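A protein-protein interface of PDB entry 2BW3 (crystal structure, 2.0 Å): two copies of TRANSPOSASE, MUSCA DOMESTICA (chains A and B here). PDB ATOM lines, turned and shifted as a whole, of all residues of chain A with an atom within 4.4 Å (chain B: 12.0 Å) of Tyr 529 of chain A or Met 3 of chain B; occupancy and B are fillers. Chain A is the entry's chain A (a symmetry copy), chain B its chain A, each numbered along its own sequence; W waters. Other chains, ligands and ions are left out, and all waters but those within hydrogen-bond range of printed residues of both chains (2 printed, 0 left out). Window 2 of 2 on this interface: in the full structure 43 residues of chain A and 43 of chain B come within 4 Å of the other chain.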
ATOM      1  N   ASP A  79     -31.674 -27.676  12.867  1.00  0.00           N
ATOM      2  CA  ASP A  79     -31.075 -26.665  13.767  1.00  0.00           C
ATOM      3  C   ASP A  79     -29.798 -27.251  14.413  1.00  0.00           C
ATOM      4  O   ASP A  79     -28.778 -26.570  14.535  1.00  0.00           O
ATOM      5  CB  ASP A  79     -32.045 -26.250  14.891  1.00  0.00           C
ATOM      6  CG  ASP A  79     -33.005 -25.130  14.482  1.00  0.00           C
ATOM      7  OD1 ASP A  79     -32.904 -24.577  13.368  1.00  0.00           O
ATOM      8  OD2 ASP A  79     -33.869 -24.780  15.309  1.00  0.00           O
ATOM      9  N   LYS A  83     -26.058 -25.592  14.437  1.00  0.00           N
ATOM     10  CA  LYS A  83     -25.271 -25.296  15.644  1.00  0.00           C
ATOM     11  C   LYS A  83     -23.927 -26.067  15.676  1.00  0.00           C
ATOM     12  O   LYS A  83     -22.895 -25.529  16.117  1.00  0.00           O
ATOM     13  CB  LYS A  83     -26.096 -25.549  16.906  1.00  0.00           C
ATOM     14  CG  LYS A  83     -27.458 -24.825  16.926  1.00  0.00           C
ATOM     15  CD  LYS A  83     -27.330 -23.326  16.589  1.00  0.00           C
ATOM     16  CE  LYS A  83     -28.699 -22.655  16.650  1.00  0.00           C
ATOM     17  NZ  LYS A  83     -28.654 -21.203  16.339  1.00  0.00           N
ATOM     18  N   LEU A 525     -28.715 -29.972  21.147  1.00  0.00           N
ATOM     19  CA  LEU A 525     -29.315 -28.655  20.999  1.00  0.00           C
ATOM     20  C   LEU A 525     -29.687 -28.049  22.334  1.00  0.00           C
ATOM     21  O   LEU A 525     -29.441 -26.851  22.563  1.00  0.00           O
ATOM     22  CB  LEU A 525     -30.533 -28.789  20.092  1.00  0.00           C
ATOM     23  CG  LEU A 525     -30.992 -27.628  19.227  1.00  0.00           C
ATOM     24  CD1 LEU A 525     -29.817 -26.857  18.610  1.00  0.00           C
ATOM     25  CD2 LEU A 525     -31.901 -28.237  18.169  1.00  0.00           C
ATOM     26  N   ASN A 526     -30.238 -28.879  23.221  1.00  0.00           N
ATOM     27  CA  ASN A 526     -30.618 -28.459  24.580  1.00  0.00           C
ATOM     28  C   ASN A 526     -29.327 -28.000  25.291  1.00  0.00           C
ATOM     29  O   ASN A 526     -29.292 -26.948  25.934  1.00  0.00           O
ATOM     30  CB  ASN A 526     -31.263 -29.665  25.314  1.00  0.00           C
ATOM     31  CG  ASN A 526     -31.572 -29.405  26.807  1.00  0.00           C
ATOM     32  OD1 ASN A 526     -30.671 -29.301  27.638  1.00  0.00           O
ATOM     33  ND2 ASN A 526     -32.845 -29.379  27.149  1.00  0.00           N
ATOM     34  N   SER A 527     -28.241 -28.770  25.163  1.00  0.00           N
ATOM     35  CA  SER A 527     -27.035 -28.343  25.847  1.00  0.00           C
ATOM     36  C   SER A 527     -26.441 -27.095  25.177  1.00  0.00           C
ATOM     37  O   SER A 527     -25.855 -26.247  25.855  1.00  0.00           O
ATOM     38  CB  SER A 527     -26.028 -29.523  26.015  1.00  0.00           C
ATOM     39  OG  SER A 527     -25.389 -29.825  24.809  1.00  0.00           O
ATOM     40  N   PHE A 528     -26.637 -26.935  23.866  1.00  0.00           N
ATOM     41  CA  PHE A 528     -26.135 -25.767  23.151  1.00  0.00           C
ATOM     42  C   PHE A 528     -26.828 -24.496  23.674  1.00  0.00           C
ATOM     43  O   PHE A 528     -26.164 -23.494  23.970  1.00  0.00           O
ATOM     44  CB  PHE A 528     -26.362 -25.881  21.623  1.00  0.00           C
ATOM     45  CG  PHE A 528     -25.963 -24.653  20.858  1.00  0.00           C
ATOM     46  CD1 PHE A 528     -24.666 -24.512  20.374  1.00  0.00           C
ATOM     47  CD2 PHE A 528     -26.856 -23.607  20.665  1.00  0.00           C
ATOM     48  CE1 PHE A 528     -24.264 -23.342  19.716  1.00  0.00           C
ATOM     49  CE2 PHE A 528     -26.459 -22.454  20.023  1.00  0.00           C
ATOM     50  CZ  PHE A 528     -25.144 -22.324  19.545  1.00  0.00           C
ATOM     51  N   TYR A 529     -28.155 -24.534  23.762  1.00  0.00           N
ATOM     52  CA  TYR A 529     -28.927 -23.387  24.264  1.00  0.00           C
ATOM     53  C   TYR A 529     -28.483 -23.018  25.691  1.00  0.00           C
ATOM     54  O   TYR A 529     -28.193 -21.844  25.989  1.00  0.00           O
ATOM     55  CB  TYR A 529     -30.432 -23.711  24.277  1.00  0.00           C
ATOM     56  CG  TYR A 529     -31.079 -23.928  22.918  1.00  0.00           C
ATOM     57  CD1 TYR A 529     -32.327 -24.555  22.819  1.00  0.00           C
ATOM     58  CD2 TYR A 529     -30.495 -23.454  21.742  1.00  0.00           C
ATOM     59  CE1 TYR A 529     -32.969 -24.696  21.597  1.00  0.00           C
ATOM     60  CE2 TYR A 529     -31.146 -23.596  20.503  1.00  0.00           C
ATOM     61  CZ  TYR A 529     -32.393 -24.223  20.461  1.00  0.00           C
ATOM     62  OH  TYR A 529     -33.095 -24.345  19.285  1.00  0.00           O
ATOM     63  N   LYS A 530     -28.363 -24.034  26.544  1.00  0.00           N
ATOM     64  CA  LYS A 530     -27.963 -23.840  27.937  1.00  0.00           C
ATOM     65  C   LYS A 530     -26.570 -23.184  28.053  1.00  0.00           C
ATOM     66  O   LYS A 530     -26.307 -22.332  28.917  1.00  0.00           O
ATOM     67  CB  LYS A 530     -27.961 -25.190  28.660  1.00  0.00           C
ATOM     68  CG  LYS A 530     -27.704 -25.057  30.143  1.00  0.00           C
ATOM     69  CD  LYS A 530     -27.465 -26.387  30.841  1.00  0.00           C
ATOM     70  CE  LYS A 530     -26.080 -26.957  30.537  1.00  0.00           C
ATOM     71  NZ  LYS A 530     -25.662 -27.977  31.554  1.00  0.00           N
ATOM     72  N   ASN A 531     -25.662 -23.621  27.210  1.00  0.00           N
ATOM     73  CA  ASN A 531     -24.306 -23.083  27.226  1.00  0.00           C
ATOM     74  C   ASN A 531     -24.098 -21.753  26.519  1.00  0.00           C
ATOM     75  O   ASN A 531     -23.391 -20.868  27.020  1.00  0.00           O
ATOM     76  CB  ASN A 531     -23.350 -24.094  26.580  1.00  0.00           C
ATOM     77  CG  ASN A 531     -22.923 -25.162  27.536  1.00  0.00           C
ATOM     78  OD1 ASN A 531     -21.974 -24.968  28.300  1.00  0.00           O
ATOM     79  ND2 ASN A 531     -23.644 -26.279  27.551  1.00  0.00           N
ATOM     80  N   PHE A 532     -24.689 -21.611  25.341  1.00  0.00           N
ATOM     81  CA  PHE A 532     -24.424 -20.424  24.533  1.00  0.00           C
ATOM     82  C   PHE A 532     -25.512 -19.389  24.376  1.00  0.00           C
ATOM     83  O   PHE A 532     -25.244 -18.308  23.857  1.00  0.00           O
ATOM     84  CB  PHE A 532     -23.986 -20.836  23.120  1.00  0.00           C
ATOM     85  CG  PHE A 532     -22.752 -21.696  23.077  1.00  0.00           C
ATOM     86  CD1 PHE A 532     -22.849 -23.066  23.147  1.00  0.00           C
ATOM     87  CD2 PHE A 532     -21.486 -21.122  22.950  1.00  0.00           C
ATOM     88  CE1 PHE A 532     -21.710 -23.873  23.097  1.00  0.00           C
ATOM     89  CE2 PHE A 532     -20.339 -21.926  22.898  1.00  0.00           C
ATOM     90  CZ  PHE A 532     -20.455 -23.296  22.974  1.00  0.00           C
ATOM     91  N   CYS A 533     -26.729 -19.704  24.786  1.00  0.00           N
ATOM     92  CA  CYS A 533     -27.826 -18.764  24.602  1.00  0.00           C
ATOM     93  C   CYS A 533     -28.448 -18.313  25.916  1.00  0.00           C
ATOM     94  O   CYS A 533     -29.645 -18.056  25.963  1.00  0.00           O
ATOM     95  CB  CYS A 533     -28.898 -19.397  23.696  1.00  0.00           C
ATOM     96  SG  CYS A 533     -28.242 -20.035  22.119  1.00  0.00           S
ATOM     97  N   LYS A 534     -27.630 -18.182  26.959  1.00  0.00           N
ATOM     98  CA  LYS A 534     -28.087 -17.757  28.296  1.00  0.00           C
ATOM     99  C   LYS A 534     -28.936 -18.833  28.986  1.00  0.00           C
ATOM    100  O   LYS A 534     -29.472 -18.622  30.088  1.00  0.00           O
ATOM    101  CB  LYS A 534     -28.889 -16.445  28.218  1.00  0.00           C
ATOM    102  CG  LYS A 534     -28.197 -15.359  27.439  1.00  0.00           C
ATOM    103  CD  LYS A 534     -29.135 -14.205  27.155  1.00  0.00           C
ATOM    104  CE  LYS A 534     -28.413 -13.105  26.405  1.00  0.00           C
ATOM    105  NZ  LYS A 534     -27.253 -12.565  27.185  1.00  0.00           N
ATOM    106  N   SER B   1     -30.508 -15.071  24.104  1.00  0.00           N
ATOM    107  CA  SER B   1     -31.502 -16.052  23.673  1.00  0.00           C
ATOM    108  C   SER B   1     -31.532 -16.232  22.151  1.00  0.00           C
ATOM    109  O   SER B   1     -32.580 -16.527  21.569  1.00  0.00           O
ATOM    110  CB  SER B   1     -32.888 -15.663  24.198  1.00  0.00           C
ATOM    111  OG  SER B   1     -32.897 -15.617  25.616  1.00  0.00           O
ATOM    112  N   HIS B   2     -30.368 -16.071  21.518  1.00  0.00           N
ATOM    113  CA  HIS B   2     -30.229 -16.221  20.065  1.00  0.00           C
ATOM    114  C   HIS B   2     -30.114 -17.680  19.645  1.00  0.00           C
ATOM    115  O   HIS B   2     -29.134 -18.114  19.025  1.00  0.00           O
ATOM    116  CB  HIS B   2     -29.054 -15.399  19.536  1.00  0.00           C
ATOM    117  CG  HIS B   2     -29.282 -13.923  19.611  1.00  0.00           C
ATOM    118  ND1 HIS B   2     -29.236 -13.104  18.502  1.00  0.00           N
ATOM    119  CD2 HIS B   2     -29.600 -13.122  20.656  1.00  0.00           C
ATOM    120  CE1 HIS B   2     -29.518 -11.864  18.861  1.00  0.00           C
ATOM    121  NE2 HIS B   2     -29.744 -11.849  20.163  1.00  0.00           N
ATOM    122  N   MET B   3     -31.141 -18.426  20.023  1.00  0.00           N
ATOM    123  CA  MET B   3     -31.273 -19.832  19.709  1.00  0.00           C
ATOM    124  C   MET B   3     -31.519 -19.937  18.213  1.00  0.00           C
ATOM    125  O   MET B   3     -31.126 -20.909  17.577  1.00  0.00           O
ATOM    126  CB  MET B   3     -32.458 -20.391  20.473  1.00  0.00           C
ATOM    127  CG  MET B   3     -32.294 -20.177  21.950  1.00  0.00           C
ATOM    128  SD  MET B   3     -33.816 -20.787  22.920  1.00  0.00           S
ATOM    129  CE  MET B   3     -34.419 -19.064  23.596  1.00  0.00           C
ATOM    130  N   GLN B   4     -32.181 -18.929  17.657  1.00  0.00           N
ATOM    131  CA  GLN B   4     -32.445 -18.911  16.229  1.00  0.00           C
ATOM    132  C   GLN B   4     -31.464 -17.943  15.566  1.00  0.00           C
ATOM    133  O   GLN B   4     -31.262 -16.834  16.063  1.00  0.00           O
ATOM    134  CB  GLN B   4     -33.897 -18.488  15.966  1.00  0.00           C
ATOM    135  CG  GLN B   4     -34.285 -18.520  14.500  1.00  0.00           C
ATOM    136  CD  GLN B   4     -33.838 -19.796  13.818  1.00  0.00           C
ATOM    137  OE1 GLN B   4     -32.921 -19.783  12.992  1.00  0.00           O
ATOM    138  NE2 GLN B   4     -34.430 -20.913  14.209  1.00  0.00           N
ATOM    139  N   SER B   5     -30.861 -18.373  14.460  1.00  0.00           N
ATOM    140  CA  SER B   5     -29.903 -17.566  13.701  1.00  0.00           C
ATOM    141  C   SER B   5     -30.347 -16.121  13.368  1.00  0.00           C
ATOM    142  O   SER B   5     -29.565 -15.180  13.530  1.00  0.00           O
ATOM    143  CB  SER B   5     -29.513 -18.303  12.415  1.00  0.00           C
ATOM    144  OG  SER B   5     -30.642 -18.556  11.583  1.00  0.00           O
ATOM    145  N   ARG B   6     -31.576 -15.947  12.879  1.00  0.00           N
ATOM    146  CA  ARG B   6     -32.104 -14.613  12.542  1.00  0.00           C
ATOM    147  C   ARG B   6     -31.485 -13.946  11.306  1.00  0.00           C
ATOM    148  O   ARG B   6     -30.717 -12.990  11.423  1.00  0.00           O
ATOM    149  CB  ARG B   6     -31.970 -13.638  13.721  1.00  0.00           C
ATOM    150  CG  ARG B   6     -32.607 -14.083  15.024  1.00  0.00           C
ATOM    151  CD  ARG B   6     -32.426 -13.010  16.089  1.00  0.00           C
ATOM    152  NE  ARG B   6     -32.394 -13.561  17.443  1.00  0.00           N
ATOM    153  CZ  ARG B   6     -33.027 -13.031  18.485  1.00  0.00           C
ATOM    154  NH1 ARG B   6     -33.755 -11.932  18.335  1.00  0.00           N
ATOM    155  NH2 ARG B   6     -32.906 -13.583  19.686  1.00  0.00           N
ATOM    156  N   GLU B   7     -31.838 -14.427  10.119  1.00  0.00           N
ATOM    157  CA  GLU B   7     -31.330 -13.837   8.882  1.00  0.00           C
ATOM    158  C   GLU B   7     -32.190 -12.615   8.529  1.00  0.00           C
ATOM    159  O   GLU B   7     -33.417 -12.642   8.685  1.00  0.00           O
ATOM    160  CB  GLU B   7     -31.384 -14.847   7.724  1.00  0.00           C
ATOM    161  CG  GLU B   7     -30.238 -15.866   7.670  1.00  0.00           C
ATOM    162  CD  GLU B   7     -30.239 -16.849   8.833  1.00  0.00           C
ATOM    163  OE1 GLU B   7     -29.212 -16.917   9.542  1.00  0.00           O
ATOM    164  OE2 GLU B   7     -31.253 -17.560   9.029  1.00  0.00           O
HETATM  165  O   HOH W   1     -34.980 -22.270  16.336  1.00  0.00           O
HETATM  166  O   HOH W   2     -31.981 -23.184  17.195  1.00  0.00           O
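The side-chain sulfur (SG) of Cys 533 of chain A is in hydrogen-bond range of the backbone carbonyl oxygen (O) of His 2 of chain B (3.7 Å). The backbone carbonyl oxygen (O) of Met 3 of chain B lies within hydrogen-bond range of the side-chain amino group (NZ) of Lys 83 of chain A, at 2.8 Å.
Of the 12 printed residues of chain A, 4 touch a printed residue of chain B. Hydrophobic or aromatic side chains of chain A within 4 Å of the printed part of chain B: Tyr 529. Along chain A the printed residues that touch a printed residue of chain B span positions 83 to 534. Hydrophobic or aromatic side chains of chain B that line the printed part of chain A: Met 3. Among the printed residues, 6 pairs touch across the chains.
No position is printed for both chains. Of the 6 pairs that touch across the chains among the printed residues, none has its exchanged pair printed and touching as well.
Water W2 lies within hydrogen-bond range of the backbone carbonyl oxygen of Met 3 of chain B (2.5 Å), the side-chain hydroxyl of Tyr 529 of chain A (2.6 Å) and the side-chain carboxylate of Asp 79 of chain A (3.1 Å). Water W1 lies within hydrogen-bond range of NE2 of Gln 4 of chain B (2.6 Å) and OD2 of Asp 79 of chain A (2.9 Å).
No residue of chain B comes within 4 Å of Asp 79 of chain A. Of the printed residues of chain B, Lys 83 of chain A touches Met 3. No residue of chain B comes within 4 Å of Leu 525 of chain A. Of chain B, only Met 3 (3.5 Å) comes within 4 Å of Tyr 529 of chain A. No residue of chain B comes within 4 Å of Asn 531 of chain A. Of the printed residues of chain B, Cys 533 of chain A touches Ser 1 (3.6 Å), His 2 (3.7 Å) and Met 3 (3.9 Å). Of the printed residues of chain A, Ser 1 of chain B touches Cys 533 and Lys 534. Printed residues of chain A within 4 Å of His 2 of chain B: Cys 533. Met 3 of chain B touches three residues of chain A. Gln 4 of chain B touches none of the printed residues of chain A. The nearest printed residue of chain A that does not touch Ser 1 of chain B is Phe 532 of chain A (6.2 Å).
Among the printed residues, pairs that only touch across the chains: Tyr 529 of chain A with Met 3 of chain B (3.5 Å), Cys 533 of chain A with Ser 1 of chain B (3.6 Å), Cys 533 of chain A with Met 3 of chain B (3.9 Å) and Lys 534 of chain A with Ser 1 of chain B (3.5 Å).
NE of Arg 6 of chain B is in hydrogen-bond range of ND1 of His 2 of chain B (3.4 Å).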
